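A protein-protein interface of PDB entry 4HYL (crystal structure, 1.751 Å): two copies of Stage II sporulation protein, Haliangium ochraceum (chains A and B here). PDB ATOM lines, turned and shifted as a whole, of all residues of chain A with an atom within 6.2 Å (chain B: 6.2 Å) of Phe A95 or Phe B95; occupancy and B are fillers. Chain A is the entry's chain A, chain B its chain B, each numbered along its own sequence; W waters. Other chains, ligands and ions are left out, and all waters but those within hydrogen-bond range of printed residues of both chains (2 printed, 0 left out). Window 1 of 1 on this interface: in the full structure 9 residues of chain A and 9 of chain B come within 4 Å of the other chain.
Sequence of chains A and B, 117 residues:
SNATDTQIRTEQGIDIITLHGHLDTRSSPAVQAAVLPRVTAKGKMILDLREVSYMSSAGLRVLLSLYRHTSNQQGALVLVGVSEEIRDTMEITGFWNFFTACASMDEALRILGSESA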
ATOM      1  N   LEU A  60     -16.613  32.708 -29.943  1.00  0.00           N
ATOM      2  CA  LEU A  60     -15.847  31.553 -29.490  1.00  0.00           C
ATOM      3  C   LEU A  60     -15.284  30.847 -30.703  1.00  0.00           C
ATOM      4  O   LEU A  60     -14.193  30.289 -30.664  1.00  0.00           O
ATOM      5  CB  LEU A  60     -16.726  30.615 -28.655  1.00  0.00           C
ATOM      6  CG  LEU A  60     -17.263  31.239 -27.356  1.00  0.00           C
ATOM      7  CD1 LEU A  60     -18.630  30.707 -26.960  1.00  0.00           C
ATOM      8  CD2 LEU A  60     -16.287  31.090 -26.202  1.00  0.00           C
ATOM      9  N   LEU A  64     -11.329  29.626 -31.434  1.00  0.00           N
ATOM     10  CA  LEU A  64     -11.001  28.310 -31.970  1.00  0.00           C
ATOM     11  C   LEU A  64     -10.301  28.451 -33.309  1.00  0.00           C
ATOM     12  O   LEU A  64      -9.280  27.814 -33.565  1.00  0.00           O
ATOM     13  CB  LEU A  64     -12.250  27.441 -32.110  1.00  0.00           C
ATOM     14  CG  LEU A  64     -12.794  26.862 -30.813  1.00  0.00           C
ATOM     15  CD1 LEU A  64     -13.931  25.908 -31.107  1.00  0.00           C
ATOM     16  CD2 LEU A  64     -11.684  26.149 -30.062  1.00  0.00           C
ATOM     17  N   ARG A  68      -6.615  27.084 -34.023  1.00  0.00           N
ATOM     18  CA  ARG A  68      -6.300  26.099 -35.057  1.00  0.00           C
ATOM     19  C   ARG A  68      -5.200  26.521 -36.021  1.00  0.00           C
ATOM     20  O   ARG A  68      -4.545  25.677 -36.625  1.00  0.00           O
ATOM     21  CB  ARG A  68      -7.536  25.751 -35.880  1.00  0.00           C
ATOM     22  CG  ARG A  68      -8.380  24.645 -35.325  1.00  0.00           C
ATOM     23  CD  ARG A  68      -9.414  24.208 -36.348  1.00  0.00           C
ATOM     24  NE  ARG A  68      -8.778  23.643 -37.531  1.00  0.00           N
ATOM     25  CZ  ARG A  68      -8.884  24.159 -38.746  1.00  0.00           C
ATOM     26  NH1 ARG A  68      -9.613  25.244 -38.933  1.00  0.00           N
ATOM     27  NH2 ARG A  68      -8.268  23.586 -39.771  1.00  0.00           N
ATOM     28  N   THR A  89     -17.884  29.020 -19.546  1.00  0.00           N
ATOM     29  CA  THR A  89     -18.631  28.705 -20.754  1.00  0.00           C
ATOM     30  C   THR A  89     -17.780  27.892 -21.716  1.00  0.00           C
ATOM     31  O   THR A  89     -18.293  27.039 -22.443  1.00  0.00           O
ATOM     32  CB  THR A  89     -19.099  29.988 -21.454  1.00  0.00           C
ATOM     33  OG1 THR A  89     -19.805  30.818 -20.517  1.00  0.00           O
ATOM     34  CG2 THR A  89     -20.005  29.650 -22.627  1.00  0.00           C
ATOM     35  N   MET A  90     -16.476  28.166 -21.716  1.00  0.00           N
ATOM     36  CA  MET A  90     -15.521  27.398 -22.512  1.00  0.00           C
ATOM     37  C   MET A  90     -15.183  26.047 -21.865  1.00  0.00           C
ATOM     38  O   MET A  90     -14.804  25.110 -22.559  1.00  0.00           O
ATOM     39  CB  MET A  90     -14.247  28.207 -22.773  1.00  0.00           C
ATOM     40  CG  MET A  90     -14.481  29.563 -23.457  1.00  0.00           C
ATOM     41  SD  MET A  90     -12.867  30.638 -23.728  1.00  0.00           S
ATOM     42  CE  MET A  90     -12.015  29.521 -25.062  1.00  0.00           C
ATOM     43  N   GLU A  91     -15.326  25.945 -20.544  1.00  0.00           N
ATOM     44  CA  GLU A  91     -15.080  24.683 -19.834  1.00  0.00           C
ATOM     45  C   GLU A  91     -16.144  23.624 -20.140  1.00  0.00           C
ATOM     46  O   GLU A  91     -15.848  22.432 -20.227  1.00  0.00           O
ATOM     47  CB  GLU A  91     -14.975  24.906 -18.317  1.00  0.00           C
ATOM     48  CG  GLU A  91     -13.686  25.591 -17.857  1.00  0.00           C
ATOM     49  CD  GLU A  91     -13.598  25.768 -16.344  1.00  0.00           C
ATOM     50  OE1 GLU A  91     -14.652  25.853 -15.684  1.00  0.00           O
ATOM     51  OE2 GLU A  91     -12.469  25.823 -15.807  1.00  0.00           O
ATOM     52  N   ILE A  92     -17.382  24.070 -20.295  1.00  0.00           N
ATOM     53  CA  ILE A  92     -18.505  23.187 -20.576  1.00  0.00           C
ATOM     54  C   ILE A  92     -18.362  22.500 -21.918  1.00  0.00           C
ATOM     55  O   ILE A  92     -18.576  21.296 -22.053  1.00  0.00           O
ATOM     56  CB  ILE A  92     -19.810  23.982 -20.604  1.00  0.00           C
ATOM     57  CG1 ILE A  92     -20.182  24.428 -19.198  1.00  0.00           C
ATOM     58  CG2 ILE A  92     -20.922  23.162 -21.211  1.00  0.00           C
ATOM     59  CD1 ILE A  92     -21.520  25.095 -19.132  1.00  0.00           C
ATOM     60  N   THR A  93     -18.006  23.290 -22.919  1.00  0.00           N
ATOM     61  CA  THR A  93     -17.909  22.809 -24.286  1.00  0.00           C
ATOM     62  C   THR A  93     -16.658  21.952 -24.491  1.00  0.00           C
ATOM     63  O   THR A  93     -16.635  21.063 -25.339  1.00  0.00           O
ATOM     64  CB  THR A  93     -17.928  23.987 -25.267  1.00  0.00           C
ATOM     65  OG1 THR A  93     -16.746  24.769 -25.089  1.00  0.00           O
ATOM     66  CG2 THR A  93     -19.150  24.870 -25.011  1.00  0.00           C
ATOM     67  N   GLY A  94     -15.629  22.212 -23.693  1.00  0.00           N
ATOM     68  CA  GLY A  94     -14.398  21.450 -23.767  1.00  0.00           C
ATOM     69  C   GLY A  94     -13.342  22.190 -24.559  1.00  0.00           C
ATOM     70  O   GLY A  94     -12.281  21.649 -24.864  1.00  0.00           O
ATOM     71  N   PHE A  95     -13.639  23.438 -24.889  1.00  0.00           N
ATOM     72  CA  PHE A  95     -12.738  24.251 -25.690  1.00  0.00           C
ATOM     73  C   PHE A  95     -11.661  24.878 -24.841  1.00  0.00           C
ATOM     74  O   PHE A  95     -10.581  25.187 -25.322  1.00  0.00           O
ATOM     75  CB  PHE A  95     -13.529  25.320 -26.415  1.00  0.00           C
ATOM     76  CG  PHE A  95     -14.473  24.762 -27.420  1.00  0.00           C
ATOM     77  CD1 PHE A  95     -14.174  23.576 -28.068  1.00  0.00           C
ATOM     78  CD2 PHE A  95     -15.655  25.405 -27.713  1.00  0.00           C
ATOM     79  CE1 PHE A  95     -15.034  23.041 -28.999  1.00  0.00           C
ATOM     80  CE2 PHE A  95     -16.526  24.881 -28.646  1.00  0.00           C
ATOM     81  CZ  PHE A  95     -16.214  23.694 -29.292  1.00  0.00           C
ATOM     82  N   TRP A  96     -11.963  25.039 -23.564  1.00  0.00           N
ATOM     83  CA  TRP A  96     -11.034  25.623 -22.624  1.00  0.00           C
ATOM     84  C   TRP A  96      -9.694  24.888 -22.616  1.00  0.00           C
ATOM     85  O   TRP A  96      -8.647  25.499 -22.436  1.00  0.00           O
ATOM     86  CB  TRP A  96     -11.670  25.617 -21.236  1.00  0.00           C
ATOM     87  CG  TRP A  96     -10.836  26.234 -20.167  1.00  0.00           C
ATOM     88  CD1 TRP A  96     -10.379  25.631 -19.029  1.00  0.00           C
ATOM     89  CD2 TRP A  96     -10.356  27.579 -20.134  1.00  0.00           C
ATOM     90  NE1 TRP A  96      -9.645  26.521 -18.292  1.00  0.00           N
ATOM     91  CE2 TRP A  96      -9.616  27.726 -18.951  1.00  0.00           C
ATOM     92  CE3 TRP A  96     -10.476  28.673 -20.995  1.00  0.00           C
ATOM     93  CZ2 TRP A  96      -9.004  28.924 -18.604  1.00  0.00           C
ATOM     94  CZ3 TRP A  96      -9.869  29.854 -20.650  1.00  0.00           C
ATOM     95  CH2 TRP A  96      -9.143  29.973 -19.467  1.00  0.00           C
ATOM     96  N   ASN A  97      -9.719  23.578 -22.832  1.00  0.00           N
ATOM     97  CA  ASN A  97      -8.516  22.762 -22.639  1.00  0.00           C
ATOM     98  C   ASN A  97      -7.520  22.785 -23.776  1.00  0.00           C
ATOM     99  O   ASN A  97      -6.537  22.050 -23.763  1.00  0.00           O
ATOM    100  CB  ASN A  97      -8.897  21.327 -22.322  1.00  0.00           C
ATOM    101  CG  ASN A  97      -9.671  21.228 -21.053  1.00  0.00           C
ATOM    102  OD1 ASN A  97      -9.331  21.876 -20.066  1.00  0.00           O
ATOM    103  ND2 ASN A  97     -10.741  20.444 -21.065  1.00  0.00           N
ATOM    104  N   PHE A  98      -7.784  23.632 -24.762  1.00  0.00           N
ATOM    105  CA  PHE A  98      -6.849  23.848 -25.856  1.00  0.00           C
ATOM    106  C   PHE A  98      -5.862  24.918 -25.477  1.00  0.00           C
ATOM    107  O   PHE A  98      -4.772  25.006 -26.033  1.00  0.00           O
ATOM    108  CB  PHE A  98      -7.602  24.324 -27.088  1.00  0.00           C
ATOM    109  CG  PHE A  98      -8.163  23.221 -27.911  1.00  0.00           C
ATOM    110  CD1 PHE A  98      -7.397  22.113 -28.217  1.00  0.00           C
ATOM    111  CD2 PHE A  98      -9.454  23.292 -28.388  1.00  0.00           C
ATOM    112  CE1 PHE A  98      -7.912  21.086 -28.979  1.00  0.00           C
ATOM    113  CE2 PHE A  98      -9.974  22.267 -29.149  1.00  0.00           C
ATOM    114  CZ  PHE A  98      -9.198  21.156 -29.441  1.00  0.00           C
ATOM    115  N   PHE A  99      -6.264  25.737 -24.520  1.00  0.00           N
ATOM    116  CA  PHE A  99      -5.654  27.036 -24.337  1.00  0.00           C
ATOM    117  C   PHE A  99      -4.763  27.087 -23.114  1.00  0.00           C
ATOM    118  O   PHE A  99      -4.948  26.313 -22.177  1.00  0.00           O
ATOM    119  CB  PHE A  99      -6.745  28.110 -24.267  1.00  0.00           C
ATOM    120  CG  PHE A  99      -7.560  28.223 -25.528  1.00  0.00           C
ATOM    121  CD1 PHE A  99      -7.055  28.877 -26.645  1.00  0.00           C
ATOM    122  CD2 PHE A  99      -8.818  27.688 -25.607  1.00  0.00           C
ATOM    123  CE1 PHE A  99      -7.799  28.982 -27.819  1.00  0.00           C
ATOM    124  CE2 PHE A  99      -9.560  27.795 -26.772  1.00  0.00           C
ATOM    125  CZ  PHE A  99      -9.050  28.438 -27.873  1.00  0.00           C
ATOM    126  N   LEU B  60     -20.080  15.659 -27.262  1.00  0.00           N
ATOM    127  CA  LEU B  60     -19.207  16.294 -28.228  1.00  0.00           C
ATOM    128  C   LEU B  60     -17.872  16.626 -27.567  1.00  0.00           C
ATOM    129  O   LEU B  60     -16.821  16.574 -28.209  1.00  0.00           O
ATOM    130  CB  LEU B  60     -19.903  17.525 -28.809  1.00  0.00           C
ATOM    131  CG  LEU B  60     -21.263  17.145 -29.422  1.00  0.00           C
ATOM    132  CD1 LEU B  60     -22.209  18.330 -29.589  1.00  0.00           C
ATOM    133  CD2 LEU B  60     -21.082  16.417 -30.738  1.00  0.00           C
ATOM    134  N   ARG B  61     -17.912  16.929 -26.274  1.00  0.00           N
ATOM    135  CA  ARG B  61     -16.687  17.111 -25.504  1.00  0.00           C
ATOM    136  C   ARG B  61     -15.845  15.836 -25.573  1.00  0.00           C
ATOM    137  O   ARG B  61     -14.619  15.894 -25.538  1.00  0.00           O
ATOM    138  CB  ARG B  61     -17.002  17.477 -24.048  1.00  0.00           C
ATOM    139  CG  ARG B  61     -15.996  18.413 -23.379  1.00  0.00           C
ATOM    140  CD  ARG B  61     -16.289  18.610 -21.889  1.00  0.00           C
ATOM    141  NE  ARG B  61     -17.681  18.974 -21.650  1.00  0.00           N
ATOM    142  CZ  ARG B  61     -18.359  18.648 -20.552  1.00  0.00           C
ATOM    143  NH1 ARG B  61     -17.766  17.956 -19.597  1.00  0.00           N
ATOM    144  NH2 ARG B  61     -19.633  19.006 -20.407  1.00  0.00           N
ATOM    145  N   LEU B  63     -15.720  13.790 -28.248  1.00  0.00           N
ATOM    146  CA  LEU B  63     -15.060  13.887 -29.538  1.00  0.00           C
ATOM    147  C   LEU B  63     -13.924  14.871 -29.436  1.00  0.00           C
ATOM    148  O   LEU B  63     -12.973  14.812 -30.203  1.00  0.00           O
ATOM    149  CB  LEU B  63     -16.022  14.380 -30.608  1.00  0.00           C
ATOM    150  CG  LEU B  63     -16.984  13.366 -31.203  1.00  0.00           C
ATOM    151  CD1 LEU B  63     -17.901  14.050 -32.189  1.00  0.00           C
ATOM    152  CD2 LEU B  63     -16.224  12.251 -31.870  1.00  0.00           C
ATOM    153  N   LEU B  64     -14.033  15.800 -28.494  1.00  0.00           N
ATOM    154  CA  LEU B  64     -13.030  16.849 -28.365  1.00  0.00           C
ATOM    155  C   LEU B  64     -11.732  16.349 -27.740  1.00  0.00           C
ATOM    156  O   LEU B  64     -10.643  16.662 -28.226  1.00  0.00           O
ATOM    157  CB  LEU B  64     -13.582  18.030 -27.570  1.00  0.00           C
ATOM    158  CG  LEU B  64     -12.628  19.213 -27.402  1.00  0.00           C
ATOM    159  CD1 LEU B  64     -13.344  20.541 -27.628  1.00  0.00           C
ATOM    160  CD2 LEU B  64     -11.949  19.163 -26.036  1.00  0.00           C
ATOM    161  N   SER B  65     -11.847  15.570 -26.668  1.00  0.00           N
ATOM    162  CA  SER B  65     -10.669  15.076 -25.969  1.00  0.00           C
ATOM    163  C   SER B  65      -9.970  13.992 -26.766  1.00  0.00           C
ATOM    164  O   SER B  65      -8.777  13.751 -26.602  1.00  0.00           O
ATOM    165  CB  SER B  65     -11.040  14.541 -24.597  1.00  0.00           C
ATOM    166  OG  SER B  65      -9.862  14.200 -23.898  1.00  0.00           O
ATOM    167  N   TYR B  67      -9.868  14.230 -30.023  1.00  0.00           N
ATOM    168  CA  TYR B  67      -9.106  15.024 -30.984  1.00  0.00           C
ATOM    169  C   TYR B  67      -7.833  15.591 -30.375  1.00  0.00           C
ATOM    170  O   TYR B  67      -6.747  15.398 -30.910  1.00  0.00           O
ATOM    171  CB  TYR B  67      -9.917  16.161 -31.592  1.00  0.00           C
ATOM    172  CG  TYR B  67      -9.035  16.980 -32.489  1.00  0.00           C
ATOM    173  CD1 TYR B  67      -8.714  16.544 -33.768  1.00  0.00           C
ATOM    174  CD2 TYR B  67      -8.465  18.157 -32.039  1.00  0.00           C
ATOM    175  CE1 TYR B  67      -7.875  17.272 -34.581  1.00  0.00           C
ATOM    176  CE2 TYR B  67      -7.624  18.895 -32.844  1.00  0.00           C
ATOM    177  CZ  TYR B  67      -7.334  18.453 -34.110  1.00  0.00           C
ATOM    178  OH  TYR B  67      -6.497  19.207 -34.901  1.00  0.00           O
ATOM    179  N   THR B  89     -24.610  21.101 -35.501  1.00  0.00           N
ATOM    180  CA  THR B  89     -24.168  21.379 -34.139  1.00  0.00           C
ATOM    181  C   THR B  89     -22.679  21.700 -34.015  1.00  0.00           C
ATOM    182  O   THR B  89     -22.301  22.630 -33.306  1.00  0.00           O
ATOM    183  CB  THR B  89     -24.498  20.199 -33.225  1.00  0.00           C
ATOM    184  OG1 THR B  89     -25.921  20.060 -33.154  1.00  0.00           O
ATOM    185  CG2 THR B  89     -23.940  20.438 -31.838  1.00  0.00           C
ATOM    186  N   MET B  90     -21.837  20.925 -34.693  1.00  0.00           N
ATOM    187  CA  MET B  90     -20.396  21.160 -34.664  1.00  0.00           C
ATOM    188  C   MET B  90     -19.965  22.301 -35.584  1.00  0.00           C
ATOM    189  O   MET B  90     -18.820  22.731 -35.523  1.00  0.00           O
ATOM    190  CB  MET B  90     -19.618  19.892 -35.017  1.00  0.00           C
ATOM    191  CG  MET B  90     -19.843  18.715 -34.066  1.00  0.00           C
ATOM    192  SD  MET B  90     -18.885  17.112 -34.629  1.00  0.00           S
ATOM    193  CE  MET B  90     -17.116  17.561 -34.021  1.00  0.00           C
ATOM    194  N   GLU B  91     -20.868  22.786 -36.436  1.00  0.00           N
ATOM    195  CA  GLU B  91     -20.564  23.946 -37.282  1.00  0.00           C
ATOM    196  C   GLU B  91     -20.909  25.259 -36.579  1.00  0.00           C
ATOM    197  O   GLU B  91     -20.198  26.255 -36.732  1.00  0.00           O
ATOM    198  CB  GLU B  91     -21.265  23.851 -38.642  1.00  0.00           C
ATOM    199  CG  GLU B  91     -20.600  22.903 -39.626  1.00  0.00           C
ATOM    200  CD  GLU B  91     -21.488  22.597 -40.804  1.00  0.00           C
ATOM    201  OE1 GLU B  91     -22.614  23.124 -40.836  1.00  0.00           O
ATOM    202  OE2 GLU B  91     -21.076  21.832 -41.694  1.00  0.00           O
ATOM    203  N   ILE B  92     -22.006  25.249 -35.823  1.00  0.00           N
ATOM    204  CA  ILE B  92     -22.351  26.338 -34.912  1.00  0.00           C
ATOM    205  C   ILE B  92     -21.078  26.900 -34.312  1.00  0.00           C
ATOM    206  O   ILE B  92     -20.836  28.108 -34.304  1.00  0.00           O
ATOM    207  CB  ILE B  92     -23.172  25.819 -33.710  1.00  0.00           C
ATOM    208  CG1 ILE B  92     -24.584  25.413 -34.114  1.00  0.00           C
ATOM    209  CG2 ILE B  92     -23.258  26.868 -32.628  1.00  0.00           C
ATOM    210  CD1 ILE B  92     -25.414  24.868 -32.933  1.00  0.00           C
ATOM    211  N   THR B  93     -20.260  25.982 -33.815  1.00  0.00           N
ATOM    212  CA  THR B  93     -19.106  26.314 -32.995  1.00  0.00           C
ATOM    213  C   THR B  93     -17.794  26.399 -33.801  1.00  0.00           C
ATOM    214  O   THR B  93     -16.918  27.206 -33.493  1.00  0.00           O
ATOM    215  CB  THR B  93     -19.009  25.339 -31.771  1.00  0.00           C
ATOM    216  OG1 THR B  93     -18.369  24.118 -32.145  1.00  0.00           O
ATOM    217  CG2 THR B  93     -20.393  25.026 -31.244  1.00  0.00           C
ATOM    218  N   GLY B  94     -17.678  25.595 -34.854  1.00  0.00           N
ATOM    219  CA  GLY B  94     -16.461  25.561 -35.643  1.00  0.00           C
ATOM    220  C   GLY B  94     -15.574  24.412 -35.212  1.00  0.00           C
ATOM    221  O   GLY B  94     -14.485  24.221 -35.746  1.00  0.00           O
ATOM    222  N   PHE B  95     -16.046  23.665 -34.217  1.00  0.00           N
ATOM    223  CA  PHE B  95     -15.404  22.440 -33.766  1.00  0.00           C
ATOM    224  C   PHE B  95     -15.266  21.516 -34.966  1.00  0.00           C
ATOM    225  O   PHE B  95     -14.195  20.989 -35.257  1.00  0.00           O
ATOM    226  CB  PHE B  95     -16.282  21.787 -32.703  1.00  0.00           C
ATOM    227  CG  PHE B  95     -15.592  20.723 -31.913  1.00  0.00           C
ATOM    228  CD1 PHE B  95     -14.209  20.640 -31.899  1.00  0.00           C
ATOM    229  CD2 PHE B  95     -16.320  19.798 -31.192  1.00  0.00           C
ATOM    230  CE1 PHE B  95     -13.564  19.656 -31.177  1.00  0.00           C
ATOM    231  CE2 PHE B  95     -15.678  18.809 -30.467  1.00  0.00           C
ATOM    232  CZ  PHE B  95     -14.298  18.740 -30.466  1.00  0.00           C
ATOM    233  N   TRP B  96     -16.376  21.344 -35.666  1.00  0.00           N
ATOM    234  CA  TRP B  96     -16.423  20.593 -36.903  1.00  0.00           C
ATOM    235  C   TRP B  96     -15.147  20.729 -37.722  1.00  0.00           C
ATOM    236  O   TRP B  96     -14.732  19.799 -38.406  1.00  0.00           O
ATOM    237  CB  TRP B  96     -17.600  21.086 -37.741  1.00  0.00           C
ATOM    238  CG  TRP B  96     -17.662  20.439 -39.068  1.00  0.00           C
ATOM    239  CD1 TRP B  96     -17.399  21.006 -40.289  1.00  0.00           C
ATOM    240  CD2 TRP B  96     -17.980  19.076 -39.317  1.00  0.00           C
ATOM    241  NE1 TRP B  96     -17.547  20.069 -41.281  1.00  0.00           N
ATOM    242  CE2 TRP B  96     -17.902  18.873 -40.706  1.00  0.00           C
ATOM    243  CE3 TRP B  96     -18.330  18.001 -38.498  1.00  0.00           C
ATOM    244  CZ2 TRP B  96     -18.167  17.638 -41.290  1.00  0.00           C
ATOM    245  CZ3 TRP B  96     -18.590  16.781 -39.080  1.00  0.00           C
ATOM    246  CH2 TRP B  96     -18.507  16.609 -40.461  1.00  0.00           C
ATOM    247  N   ASN B  97     -14.530  21.898 -37.674  1.00  0.00           N
ATOM    248  CA  ASN B  97     -13.394  22.154 -38.539  1.00  0.00           C
ATOM    249  C   ASN B  97     -12.152  21.457 -38.074  1.00  0.00           C
ATOM    250  O   ASN B  97     -11.147  21.469 -38.765  1.00  0.00           O
ATOM    251  CB  ASN B  97     -13.121  23.644 -38.647  1.00  0.00           C
ATOM    252  CG  ASN B  97     -14.160  24.357 -39.440  1.00  0.00           C
ATOM    253  OD1 ASN B  97     -15.254  23.843 -39.655  1.00  0.00           O
ATOM    254  ND2 ASN B  97     -13.834  25.559 -39.882  1.00  0.00           N
ATOM    255  N   PHE B  98     -12.220  20.856 -36.893  1.00  0.00           N
ATOM    256  CA  PHE B  98     -11.080  20.126 -36.350  1.00  0.00           C
ATOM    257  C   PHE B  98     -10.934  18.769 -37.007  1.00  0.00           C
ATOM    258  O   PHE B  98      -9.854  18.197 -37.019  1.00  0.00           O
ATOM    259  CB  PHE B  98     -11.239  19.917 -34.846  1.00  0.00           C
ATOM    260  CG  PHE B  98     -10.904  21.120 -34.022  1.00  0.00           C
ATOM    261  CD1 PHE B  98      -9.595  21.383 -33.661  1.00  0.00           C
ATOM    262  CD2 PHE B  98     -11.897  21.979 -33.595  1.00  0.00           C
ATOM    263  CE1 PHE B  98      -9.283  22.487 -32.896  1.00  0.00           C
ATOM    264  CE2 PHE B  98     -11.591  23.085 -32.829  1.00  0.00           C
ATOM    265  CZ  PHE B  98     -10.281  23.339 -32.480  1.00  0.00           C
ATOM    266  N   PHE B  99     -12.030  18.260 -37.557  1.00  0.00           N
ATOM    267  CA  PHE B  99     -12.106  16.862 -37.957  1.00  0.00           C
ATOM    268  C   PHE B  99     -12.018  16.613 -39.463  1.00  0.00           C
ATOM    269  O   PHE B  99     -12.155  17.535 -40.278  1.00  0.00           O
ATOM    270  CB  PHE B  99     -13.382  16.242 -37.394  1.00  0.00           C
ATOM    271  CG  PHE B  99     -13.450  16.279 -35.901  1.00  0.00           C
ATOM    272  CD1 PHE B  99     -12.928  15.241 -35.141  1.00  0.00           C
ATOM    273  CD2 PHE B  99     -14.010  17.350 -35.247  1.00  0.00           C
ATOM    274  CE1 PHE B  99     -12.974  15.286 -33.769  1.00  0.00           C
ATOM    275  CE2 PHE B  99     -14.060  17.384 -33.873  1.00  0.00           C
ATOM    276  CZ  PHE B  99     -13.544  16.360 -33.137  1.00  0.00           C
HETATM  277  O   HOH W   1     -11.708  25.973 -36.228  1.00  0.00           O
HETATM  278  O   HOH W   2      -7.253  21.174 -37.547  1.00  0.00           O
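The backbone carbonyl oxygen of Met A90 lies within hydrogen-bond range of the side-chain hydroxyl of Thr A93, 3.2 Å away. The backbone carbonyl oxygen (O) of Met A90 sits at hydrogen-bond distance from the backbone NH (N) of Phe A95 (3.1 Å). OG1 of Thr A93 lies close to N of Phe A95, 3.4 Å away. O of Met B90 sits at hydrogen-bond distance from N of Phe B95 (3.2 Å). The backbone NH of Phe B95 lies within hydrogen-bond range of the side-chain hydroxyl of Thr B93, at 3.1 Å.
Among the printed residues, merely in contact across the chains: Gly A94 with Leu B64 (2.8 Å), Phe A95 with Leu B64 (3.2 Å), Thr A93 with Arg B61 (3.4 Å), Arg A68 with Phe B98 (3.4 Å), Gly A94 with Arg B61 (3.5 Å), Phe A98 with Phe B98 (3.5 Å), Phe A95 with Thr B93 (3.6 Å), Phe A95 with Phe B95 (3.8 Å) and Leu A64 with Phe B98 (3.96 Å).
Leu A64 touches Phe B98, but with the chains exchanged Phe A98 does not touch Leu B64 (4.1 Å). Gly A94 touches Leu B64, but with the chains exchanged Leu A64 does not touch Gly B94 (4.7 Å). Phe A95 touches Leu B64, but with the chains exchanged Leu A64 does not touch Phe B95 (4.4 Å). Phe A95 touches Thr B93, but with the chains exchanged Thr A93 does not touch Phe B95 (5.7 Å). Positions printed for both chains: 60, 64, 89, 90, 91, 92, 93, 94, 95, 96, 97, 98 and 99. Of the 11 pairs that touch across the chains among the printed residues, 2 have their exchanged pair printed and touching as well.
Water W2 lies within hydrogen-bond range of NE of Arg A68 and OH of Tyr B67. Water W1 bridges the backbone carbonyl oxygen of Gly B94 (3.3 Å) and the guanidinium group of Arg A68 (3.5 Å).
Of chain B, only Leu B64 (3.2 Å), Thr B93 (3.6 Å) and Phe B95 (3.8 Å) come within 4 Å of Phe A95. Phe B95 touches just one residue of chain A: Phe A95. Printed residues of chain B within 4 Å of Leu A64: Phe B98. Printed residues of chain B within 4 Å of Ile A92: Arg B61. Of the printed residues of chain A, Leu B64 touches Gly A94 (2.8 Å) and Phe A95 (3.2 Å). Printed residues of chain A within 4 Å of Arg B61: Ile A92, Thr A93 and Gly A94. Glu A91 touches none of the printed residues of chain B. Glu B91 touches none of the printed residues of chain A. The nearest residue of chain B that does not touch Phe A95 is Phe B98 (5.2 Å). The nearest residue of chain A that does not touch Phe B95 is Leu A64 (4.4 Å). The nearest printed residue of chain B that does not touch Phe A98 is Tyr B67 (4.03 Å).
Printed residues of chain B that touch a printed residue of chain A: Arg B61, Leu B64, Thr B93, Phe B95, Asn B97 and Phe B98. Hydrophobic or aromatic side chains of chain B within 4 Å of the printed part of chain A: Leu B64, Phe B95 and Phe B98. Of the 14 printed residues of chain A, 7 touch a printed residue of chain B. Printed residues of chain A that touch a printed residue of chain B: Leu A64, Arg A68, Ile A92, Thr A93, Gly A94, Phe A95 and Phe A98. Hydrophobic or aromatic side chains of chain A that line the printed part of chain B: Leu A64, Phe A95 and Phe A98. Along chain A the printed residues that touch a printed residue of chain B span positions 64 to 98. Among the printed residues, 11 pairs touch across the chains. Among the printed residues, no Asp or Glu carboxylate lies within 4 Å of a Lys or Arg side-chain nitrogen of the other chain.
O of Asn B97 sits at hydrogen-bond distance from NE of Arg A68 (3.4 Å). O of Ile A92 lies within hydrogen-bond range of NE of Arg B61 (2.5 Å).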
